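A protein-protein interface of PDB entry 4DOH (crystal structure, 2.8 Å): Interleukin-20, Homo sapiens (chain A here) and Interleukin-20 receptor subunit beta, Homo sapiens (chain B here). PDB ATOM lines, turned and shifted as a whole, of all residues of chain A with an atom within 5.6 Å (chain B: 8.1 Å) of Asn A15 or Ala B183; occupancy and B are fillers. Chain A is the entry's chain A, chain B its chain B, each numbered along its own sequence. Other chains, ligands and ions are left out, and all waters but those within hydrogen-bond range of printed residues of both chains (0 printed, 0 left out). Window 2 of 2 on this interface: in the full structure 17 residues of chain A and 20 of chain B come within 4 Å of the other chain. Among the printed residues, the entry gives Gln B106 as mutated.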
ATOM      1  N   ALA A   1     -22.165  -3.547 -16.778  1.00  0.00           N
ATOM      2  CA  ALA A   1     -20.838  -3.963 -17.193  1.00  0.00           C
ATOM      3  C   ALA A   1     -20.845  -5.199 -18.075  1.00  0.00           C
ATOM      4  O   ALA A   1     -21.615  -6.137 -17.855  1.00  0.00           O
ATOM      5  N   LEU A   2     -19.994  -5.186 -19.095  1.00  0.00           N
ATOM      6  CA  LEU A   2     -19.766  -6.360 -19.940  1.00  0.00           C
ATOM      7  C   LEU A   2     -19.047  -7.472 -19.171  1.00  0.00           C
ATOM      8  O   LEU A   2     -18.473  -7.236 -18.097  1.00  0.00           O
ATOM      9  CB  LEU A   2     -18.921  -5.984 -21.162  1.00  0.00           C
ATOM     10  CG  LEU A   2     -19.630  -5.156 -22.228  1.00  0.00           C
ATOM     11  CD1 LEU A   2     -18.625  -4.693 -23.280  1.00  0.00           C
ATOM     12  CD2 LEU A   2     -20.748  -5.983 -22.848  1.00  0.00           C
ATOM     13  N   LYS A   3     -19.065  -8.681 -19.726  1.00  0.00           N
ATOM     14  CA  LYS A   3     -18.308  -9.776 -19.142  1.00  0.00           C
ATOM     15  C   LYS A   3     -17.020  -9.998 -19.924  1.00  0.00           C
ATOM     16  O   LYS A   3     -17.039 -10.269 -21.125  1.00  0.00           O
ATOM     17  CB  LYS A   3     -19.138 -11.052 -19.086  1.00  0.00           C
ATOM     18  CG  LYS A   3     -18.434 -12.203 -18.401  1.00  0.00           C
ATOM     19  CD  LYS A   3     -17.997 -11.824 -16.993  1.00  0.00           C
ATOM     20  CE  LYS A   3     -17.423 -13.019 -16.242  1.00  0.00           C
ATOM     21  NZ  LYS A   3     -16.423 -13.737 -17.067  1.00  0.00           N
ATOM     22  N   ALA A  13     -15.143  -9.461 -25.056  1.00  0.00           N
ATOM     23  CA  ALA A  13     -16.127  -8.809 -24.225  1.00  0.00           C
ATOM     24  C   ALA A  13     -17.515  -9.289 -24.660  1.00  0.00           C
ATOM     25  O   ALA A  13     -17.855  -9.247 -25.838  1.00  0.00           O
ATOM     26  CB  ALA A  13     -16.002  -7.320 -24.390  1.00  0.00           C
ATOM     27  N   THR A  14     -18.309  -9.772 -23.716  1.00  0.00           N
ATOM     28  CA  THR A  14     -19.623 -10.312 -24.050  1.00  0.00           C
ATOM     29  C   THR A  14     -20.732  -9.639 -23.241  1.00  0.00           C
ATOM     30  O   THR A  14     -20.535  -9.235 -22.100  1.00  0.00           O
ATOM     31  CB  THR A  14     -19.691 -11.848 -23.835  1.00  0.00           C
ATOM     32  OG1 THR A  14     -19.669 -12.139 -22.432  1.00  0.00           O
ATOM     33  CG2 THR A  14     -18.513 -12.561 -24.508  1.00  0.00           C
ATOM     34  N   ASN A  15     -21.900  -9.508 -23.850  1.00  0.00           N
ATOM     35  CA  ASN A  15     -23.055  -8.979 -23.144  1.00  0.00           C
ATOM     36  C   ASN A  15     -23.887 -10.102 -22.520  1.00  0.00           C
ATOM     37  O   ASN A  15     -25.028 -10.356 -22.921  1.00  0.00           O
ATOM     38  CB  ASN A  15     -23.916  -8.122 -24.064  1.00  0.00           C
ATOM     39  CG  ASN A  15     -24.763  -7.140 -23.300  1.00  0.00           C
ATOM     40  OD1 ASN A  15     -24.943  -7.268 -22.077  1.00  0.00           O
ATOM     41  ND2 ASN A  15     -25.292  -6.146 -24.007  1.00  0.00           N
ATOM     42  N   LEU A  16     -23.298 -10.783 -21.545  1.00  0.00           N
ATOM     43  CA  LEU A  16     -24.004 -11.832 -20.840  1.00  0.00           C
ATOM     44  C   LEU A  16     -25.359 -11.375 -20.298  1.00  0.00           C
ATOM     45  O   LEU A  16     -26.321 -12.138 -20.320  1.00  0.00           O
ATOM     46  CB  LEU A  16     -23.143 -12.370 -19.710  1.00  0.00           C
ATOM     47  CG  LEU A  16     -22.639 -13.779 -19.986  1.00  0.00           C
ATOM     48  CD1 LEU A  16     -22.332 -13.952 -21.461  1.00  0.00           C
ATOM     49  CD2 LEU A  16     -21.435 -14.070 -19.119  1.00  0.00           C
ATOM     50  N   GLN A  17     -25.442 -10.130 -19.826  1.00  0.00           N
ATOM     51  CA  GLN A  17     -26.664  -9.666 -19.176  1.00  0.00           C
ATOM     52  C   GLN A  17     -27.865  -9.669 -20.113  1.00  0.00           C
ATOM     53  O   GLN A  17     -28.911 -10.228 -19.789  1.00  0.00           O
ATOM     54  CB  GLN A  17     -26.492  -8.293 -18.560  1.00  0.00           C
ATOM     55  CG  GLN A  17     -27.467  -8.095 -17.434  1.00  0.00           C
ATOM     56  CD  GLN A  17     -27.546  -9.337 -16.565  1.00  0.00           C
ATOM     57  OE1 GLN A  17     -26.525  -9.803 -16.060  1.00  0.00           O
ATOM     58  NE2 GLN A  17     -28.752  -9.896 -16.406  1.00  0.00           N
ATOM     59  N   GLU A  18     -27.700  -9.046 -21.274  1.00  0.00           N
ATOM     60  CA  GLU A  18     -28.716  -9.058 -22.316  1.00  0.00           C
ATOM     61  C   GLU A  18     -29.236 -10.471 -22.546  1.00  0.00           C
ATOM     62  O   GLU A  18     -30.436 -10.701 -22.529  1.00  0.00           O
ATOM     63  CB  GLU A  18     -28.152  -8.477 -23.610  1.00  0.00           C
ATOM     64  CG  GLU A  18     -29.168  -8.209 -24.716  1.00  0.00           C
ATOM     65  CD  GLU A  18     -28.560  -7.446 -25.900  1.00  0.00           C
ATOM     66  OE1 GLU A  18     -27.638  -7.992 -26.564  1.00  0.00           O
ATOM     67  OE2 GLU A  18     -29.000  -6.296 -26.160  1.00  0.00           O
ATOM     68  N   ILE A  19     -28.345 -11.433 -22.738  1.00  0.00           N
ATOM     69  CA  ILE A  19     -28.812 -12.792 -23.018  1.00  0.00           C
ATOM     70  C   ILE A  19     -29.575 -13.446 -21.853  1.00  0.00           C
ATOM     71  O   ILE A  19     -30.598 -14.109 -22.059  1.00  0.00           O
ATOM     72  CB  ILE A  19     -27.674 -13.720 -23.462  1.00  0.00           C
ATOM     73  CG1 ILE A  19     -26.926 -13.127 -24.647  1.00  0.00           C
ATOM     74  CG2 ILE A  19     -28.238 -15.071 -23.857  1.00  0.00           C
ATOM     75  CD1 ILE A  19     -25.599 -13.794 -24.874  1.00  0.00           C
ATOM     76  N   ARG A  20     -29.074 -13.274 -20.635  1.00  0.00           N
ATOM     77  CA  ARG A  20     -29.750 -13.829 -19.462  1.00  0.00           C
ATOM     78  C   ARG A  20     -31.139 -13.222 -19.268  1.00  0.00           C
ATOM     79  O   ARG A  20     -32.090 -13.935 -18.961  1.00  0.00           O
ATOM     80  CB  ARG A  20     -28.915 -13.620 -18.215  1.00  0.00           C
ATOM     81  CG  ARG A  20     -27.574 -14.288 -18.292  1.00  0.00           C
ATOM     82  CD  ARG A  20     -26.816 -14.108 -17.002  1.00  0.00           C
ATOM     83  NE  ARG A  20     -26.591 -15.393 -16.366  1.00  0.00           N
ATOM     84  CZ  ARG A  20     -25.503 -15.704 -15.675  1.00  0.00           C
ATOM     85  NH1 ARG A  20     -24.534 -14.810 -15.541  1.00  0.00           N
ATOM     86  NH2 ARG A  20     -25.386 -16.908 -15.125  1.00  0.00           N
ATOM     87  N   MET B  20     -31.089   4.635 -28.701  1.00  0.00           N
ATOM     88  CA  MET B  20     -31.428   3.221 -28.738  1.00  0.00           C
ATOM     89  C   MET B  20     -32.930   2.970 -28.776  1.00  0.00           C
ATOM     90  O   MET B  20     -33.395   1.917 -28.349  1.00  0.00           O
ATOM     91  CB  MET B  20     -30.787   2.495 -27.557  1.00  0.00           C
ATOM     92  CG  MET B  20     -29.280   2.487 -27.634  1.00  0.00           C
ATOM     93  SD  MET B  20     -28.624   1.268 -28.798  1.00  0.00           S
ATOM     94  CE  MET B  20     -28.854  -0.270 -27.851  1.00  0.00           C
ATOM     95  N   THR B  76     -32.563  -6.394 -30.906  1.00  0.00           N
ATOM     96  CA  THR B  76     -32.072  -6.652 -29.558  1.00  0.00           C
ATOM     97  C   THR B  76     -30.681  -7.250 -29.556  1.00  0.00           C
ATOM     98  O   THR B  76     -30.254  -7.844 -28.568  1.00  0.00           O
ATOM     99  CB  THR B  76     -32.980  -7.652 -28.837  1.00  0.00           C
ATOM    100  OG1 THR B  76     -33.024  -8.871 -29.591  1.00  0.00           O
ATOM    101  CG2 THR B  76     -34.372  -7.104 -28.695  1.00  0.00           C
ATOM    102  N   ALA B  77     -29.984  -7.116 -30.673  1.00  0.00           N
ATOM    103  CA  ALA B  77     -28.643  -7.647 -30.789  1.00  0.00           C
ATOM    104  C   ALA B  77     -27.857  -6.719 -31.706  1.00  0.00           C
ATOM    105  O   ALA B  77     -28.450  -6.069 -32.579  1.00  0.00           O
ATOM    106  CB  ALA B  77     -28.676  -9.068 -31.341  1.00  0.00           C
ATOM    107  N   THR B  78     -26.536  -6.636 -31.513  1.00  0.00           N
ATOM    108  CA  THR B  78     -25.761  -5.680 -32.290  1.00  0.00           C
ATOM    109  C   THR B  78     -25.277  -6.265 -33.619  1.00  0.00           C
ATOM    110  O   THR B  78     -24.092  -6.465 -33.849  1.00  0.00           O
ATOM    111  CB  THR B  78     -24.656  -5.002 -31.464  1.00  0.00           C
ATOM    112  OG1 THR B  78     -25.190  -4.631 -30.190  1.00  0.00           O
ATOM    113  CG2 THR B  78     -24.176  -3.729 -32.154  1.00  0.00           C
ATOM    114  N   VAL B  79     -26.251  -6.526 -34.485  1.00  0.00           N
ATOM    115  CA  VAL B  79     -26.044  -7.052 -35.825  1.00  0.00           C
ATOM    116  C   VAL B  79     -26.943  -6.297 -36.798  1.00  0.00           C
ATOM    117  O   VAL B  79     -27.868  -5.599 -36.377  1.00  0.00           O
ATOM    118  CB  VAL B  79     -26.393  -8.533 -35.884  1.00  0.00           C
ATOM    119  CG1 VAL B  79     -25.503  -9.296 -34.938  1.00  0.00           C
ATOM    120  CG2 VAL B  79     -27.877  -8.755 -35.556  1.00  0.00           C
ATOM    121  N   ASN B 104     -28.327  -1.368 -38.288  1.00  0.00           N
ATOM    122  CA  ASN B 104     -27.599  -1.804 -37.092  1.00  0.00           C
ATOM    123  C   ASN B 104     -27.670  -0.775 -35.959  1.00  0.00           C
ATOM    124  O   ASN B 104     -27.318   0.385 -36.153  1.00  0.00           O
ATOM    125  CB  ASN B 104     -26.136  -2.073 -37.417  1.00  0.00           C
ATOM    126  CG  ASN B 104     -25.440  -2.881 -36.339  1.00  0.00           C
ATOM    127  OD1 ASN B 104     -25.741  -2.750 -35.159  1.00  0.00           O
ATOM    128  ND2 ASN B 104     -24.515  -3.731 -36.746  1.00  0.00           N
ATOM    129  N   ARG B 105     -28.103  -1.196 -34.776  1.00  0.00           N
ATOM    130  CA  ARG B 105     -28.315  -0.237 -33.694  1.00  0.00           C
ATOM    131  C   ARG B 105     -27.056   0.553 -33.325  1.00  0.00           C
ATOM    132  O   ARG B 105     -27.137   1.598 -32.660  1.00  0.00           O
ATOM    133  CB  ARG B 105     -28.918  -0.909 -32.466  1.00  0.00           C
ATOM    134  CG  ARG B 105     -27.983  -1.862 -31.747  1.00  0.00           C
ATOM    135  CD  ARG B 105     -28.735  -2.535 -30.615  1.00  0.00           C
ATOM    136  NE  ARG B 105     -27.984  -3.644 -30.062  1.00  0.00           N
ATOM    137  CZ  ARG B 105     -28.423  -4.414 -29.080  1.00  0.00           C
ATOM    138  NH1 ARG B 105     -29.624  -4.211 -28.546  1.00  0.00           N
ATOM    139  NH2 ARG B 105     -27.660  -5.395 -28.638  1.00  0.00           N
ATOM    140  N   GLN B 106     -25.904   0.069 -33.788  1.00  0.00           N
ATOM    141  CA  GLN B 106     -24.618   0.740 -33.577  1.00  0.00           C
ATOM    142  C   GLN B 106     -24.639   2.194 -34.025  1.00  0.00           C
ATOM    143  O   GLN B 106     -23.757   2.976 -33.686  1.00  0.00           O
ATOM    144  CB  GLN B 106     -23.521   0.011 -34.345  1.00  0.00           C
ATOM    145  CG  GLN B 106     -22.186   0.715 -34.319  1.00  0.00           C
ATOM    146  CD  GLN B 106     -21.056  -0.232 -33.983  1.00  0.00           C
ATOM    147  OE1 GLN B 106     -21.035  -1.376 -34.447  1.00  0.00           O
ATOM    148  NE2 GLN B 106     -20.114   0.231 -33.163  1.00  0.00           N
ATOM    149  N   PRO B 133     -32.580   0.463 -19.582  1.00  0.00           N
ATOM    150  CA  PRO B 133     -31.555  -0.491 -19.143  1.00  0.00           C
ATOM    151  C   PRO B 133     -30.363  -0.597 -20.099  1.00  0.00           C
ATOM    152  O   PRO B 133     -29.316  -1.068 -19.664  1.00  0.00           O
ATOM    153  CB  PRO B 133     -32.328  -1.807 -19.029  1.00  0.00           C
ATOM    154  CG  PRO B 133     -33.473  -1.638 -19.974  1.00  0.00           C
ATOM    155  CD  PRO B 133     -33.844  -0.187 -19.950  1.00  0.00           C
ATOM    156  N   GLN B 134     -30.500  -0.146 -21.350  1.00  0.00           N
ATOM    157  CA  GLN B 134     -29.374  -0.170 -22.300  1.00  0.00           C
ATOM    158  C   GLN B 134     -28.266   0.812 -21.939  1.00  0.00           C
ATOM    159  O   GLN B 134     -27.222   0.824 -22.593  1.00  0.00           O
ATOM    160  CB  GLN B 134     -29.823   0.169 -23.725  1.00  0.00           C
ATOM    161  CG  GLN B 134     -30.620  -0.884 -24.445  1.00  0.00           C
ATOM    162  CD  GLN B 134     -29.903  -2.196 -24.545  1.00  0.00           C
ATOM    163  OE1 GLN B 134     -28.694  -2.274 -24.342  1.00  0.00           O
ATOM    164  NE2 GLN B 134     -30.648  -3.252 -24.848  1.00  0.00           N
ATOM    165  N   PHE B 135     -28.517   1.635 -20.918  1.00  0.00           N
ATOM    166  CA  PHE B 135     -27.693   2.804 -20.594  1.00  0.00           C
ATOM    167  C   PHE B 135     -27.096   2.808 -19.194  1.00  0.00           C
ATOM    168  O   PHE B 135     -27.758   2.466 -18.209  1.00  0.00           O
ATOM    169  CB  PHE B 135     -28.534   4.059 -20.703  1.00  0.00           C
ATOM    170  CG  PHE B 135     -28.872   4.436 -22.090  1.00  0.00           C
ATOM    171  CD1 PHE B 135     -28.081   5.322 -22.780  1.00  0.00           C
ATOM    172  CD2 PHE B 135     -29.990   3.910 -22.713  1.00  0.00           C
ATOM    173  CE1 PHE B 135     -28.395   5.685 -24.068  1.00  0.00           C
ATOM    174  CE2 PHE B 135     -30.310   4.264 -24.001  1.00  0.00           C
ATOM    175  CZ  PHE B 135     -29.510   5.158 -24.680  1.00  0.00           C
ATOM    176  N   GLU B 136     -25.849   3.249 -19.126  1.00  0.00           N
ATOM    177  CA  GLU B 136     -25.152   3.532 -17.869  1.00  0.00           C
ATOM    178  C   GLU B 136     -24.622   4.973 -17.938  1.00  0.00           C
ATOM    179  O   GLU B 136     -24.351   5.485 -19.021  1.00  0.00           O
ATOM    180  CB  GLU B 136     -23.993   2.544 -17.655  1.00  0.00           C
ATOM    181  CG  GLU B 136     -24.395   1.209 -17.022  1.00  0.00           C
ATOM    182  CD  GLU B 136     -23.317   0.124 -17.164  1.00  0.00           C
ATOM    183  OE1 GLU B 136     -23.469  -0.969 -16.560  1.00  0.00           O
ATOM    184  OE2 GLU B 136     -22.324   0.365 -17.892  1.00  0.00           O
ATOM    185  N   PHE B 180     -23.156   5.746 -21.346  1.00  0.00           N
ATOM    186  CA  PHE B 180     -22.424   4.679 -21.985  1.00  0.00           C
ATOM    187  C   PHE B 180     -23.367   3.522 -22.290  1.00  0.00           C
ATOM    188  O   PHE B 180     -24.001   2.937 -21.406  1.00  0.00           O
ATOM    189  CB  PHE B 180     -21.244   4.234 -21.144  1.00  0.00           C
ATOM    190  CG  PHE B 180     -20.440   3.152 -21.776  1.00  0.00           C
ATOM    191  CD1 PHE B 180     -19.617   3.427 -22.848  1.00  0.00           C
ATOM    192  CD2 PHE B 180     -20.513   1.855 -21.308  1.00  0.00           C
ATOM    193  CE1 PHE B 180     -18.877   2.444 -23.438  1.00  0.00           C
ATOM    194  CE2 PHE B 180     -19.764   0.856 -21.889  1.00  0.00           C
ATOM    195  CZ  PHE B 180     -18.944   1.149 -22.963  1.00  0.00           C
ATOM    196  N   VAL B 181     -23.478   3.230 -23.575  1.00  0.00           N
ATOM    197  CA  VAL B 181     -24.248   2.099 -24.049  1.00  0.00           C
ATOM    198  C   VAL B 181     -23.304   0.910 -24.276  1.00  0.00           C
ATOM    199  O   VAL B 181     -22.546   0.894 -25.250  1.00  0.00           O
ATOM    200  CB  VAL B 181     -24.915   2.467 -25.358  1.00  0.00           C
ATOM    201  CG1 VAL B 181     -25.629   1.279 -25.937  1.00  0.00           C
ATOM    202  CG2 VAL B 181     -25.860   3.618 -25.137  1.00  0.00           C
ATOM    203  N   LYS B 182     -23.321  -0.073 -23.380  1.00  0.00           N
ATOM    204  CA  LYS B 182     -22.338  -1.147 -23.497  1.00  0.00           C
ATOM    205  C   LYS B 182     -22.554  -1.991 -24.749  1.00  0.00           C
ATOM    206  O   LYS B 182     -21.600  -2.427 -25.380  1.00  0.00           O
ATOM    207  CB  LYS B 182     -22.205  -2.018 -22.223  1.00  0.00           C
ATOM    208  CG  LYS B 182     -23.446  -2.737 -21.741  1.00  0.00           C
ATOM    209  CD  LYS B 182     -23.097  -3.790 -20.707  1.00  0.00           C
ATOM    210  CE  LYS B 182     -24.120  -3.861 -19.570  1.00  0.00           C
ATOM    211  NZ  LYS B 182     -25.538  -3.771 -20.043  1.00  0.00           N
ATOM    212  N   ALA B 183     -23.810  -2.191 -25.124  1.00  0.00           N
ATOM    213  CA  ALA B 183     -24.120  -3.087 -26.224  1.00  0.00           C
ATOM    214  C   ALA B 183     -23.513  -2.635 -27.556  1.00  0.00           C
ATOM    215  O   ALA B 183     -23.407  -3.435 -28.480  1.00  0.00           O
ATOM    216  CB  ALA B 183     -25.615  -3.259 -26.354  1.00  0.00           C
ATOM    217  N   ILE B 184     -23.123  -1.367 -27.660  1.00  0.00           N
ATOM    218  CA  ILE B 184     -22.564  -0.823 -28.900  1.00  0.00           C
ATOM    219  C   ILE B 184     -21.222  -0.120 -28.689  1.00  0.00           C
ATOM    220  O   ILE B 184     -20.618   0.379 -29.642  1.00  0.00           O
ATOM    221  CB  ILE B 184     -23.516   0.188 -29.559  1.00  0.00           C
ATOM    222  CG1 ILE B 184     -23.626   1.454 -28.706  1.00  0.00           C
ATOM    223  CG2 ILE B 184     -24.874  -0.418 -29.754  1.00  0.00           C
ATOM    224  CD1 ILE B 184     -24.602   2.480 -29.236  1.00  0.00           C
ATOM    225  N   GLY B 185     -20.774  -0.067 -27.435  1.00  0.00           N
ATOM    226  CA  GLY B 185     -19.500   0.533 -27.083  1.00  0.00           C
ATOM    227  C   GLY B 185     -19.323   2.015 -27.398  1.00  0.00           C
ATOM    228  O   GLY B 185     -18.247   2.438 -27.831  1.00  0.00           O
ATOM    229  N   ARG B 186     -20.357   2.820 -27.175  1.00  0.00           N
ATOM    230  CA  ARG B 186     -20.243   4.242 -27.490  1.00  0.00           C
ATOM    231  C   ARG B 186     -20.713   5.146 -26.356  1.00  0.00           C
ATOM    232  O   ARG B 186     -21.590   4.779 -25.571  1.00  0.00           O
ATOM    233  CB  ARG B 186     -20.988   4.567 -28.777  1.00  0.00           C
ATOM    234  CG  ARG B 186     -20.503   3.774 -29.981  1.00  0.00           C
ATOM    235  CD  ARG B 186     -21.279   4.166 -31.218  1.00  0.00           C
ATOM    236  NE  ARG B 186     -21.570   5.605 -31.258  1.00  0.00           N
ATOM    237  CZ  ARG B 186     -22.710   6.133 -31.703  1.00  0.00           C
ATOM    238  NH1 ARG B 186     -23.685   5.352 -32.151  1.00  0.00           N
ATOM    239  NH2 ARG B 186     -22.889   7.445 -31.701  1.00  0.00           N
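OD1 of Asn A15 lies within hydrogen-bond range of N of Glu A18, at 3.4 Å. The guanidinium group (NE) of Arg B105 lies within hydrogen-bond range of the side-chain hydroxyl (OG1) of Thr B78. The side-chain hydroxyl of Thr B78 is in hydrogen-bond range of the backbone carbonyl oxygen of Ala B183 (2.7 Å). O of Glu B136 is in hydrogen-bond range of N of Phe B180 (2.6 Å).
The backbone NH of Ala A1 is in hydrogen-bond range of the side-chain carboxylate of Glu B136 (2.9 Å). The guanidinium group (NH2) of Arg B105 lies within salt-bridge range of the side-chain carboxylate (OE2) of Glu A18, 3.0 Å away. The side-chain carboxylate (OE2) of Glu A18 lies close to the backbone carbonyl oxygen (O) of Thr B76, at 3.1 Å.
Among the printed residues, Asp or Glu carboxylates within 4 Å of a Lys or Arg side-chain nitrogen of the other chain: Glu A18 with Arg B105 (3.0 Å).
Lys B182 touches Ala A1. Lys B182 touches Leu A2. Asn A15 touches Ala B183 (ND2 to CB, 3.7 Å). Glu A18 touches Gln B134.
Printed residues of chain B within 4 Å of Ala A1: Glu B136 (2.9 Å) and Lys B182 (3.4 Å). Of chain B, only Ala B183 comes within 4 Å of Asn A15. Printed residues of chain A within 4 Å of Glu B136: Ala A1. Of the printed residues of chain A, Ala B183 touches Asn A15. The nearest residue of chain A that does not touch Ala B183 is Glu A18 (4.6 Å). The nearest printed residue of chain A that does not touch Lys B182 is Asn A15 (4.1 Å).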
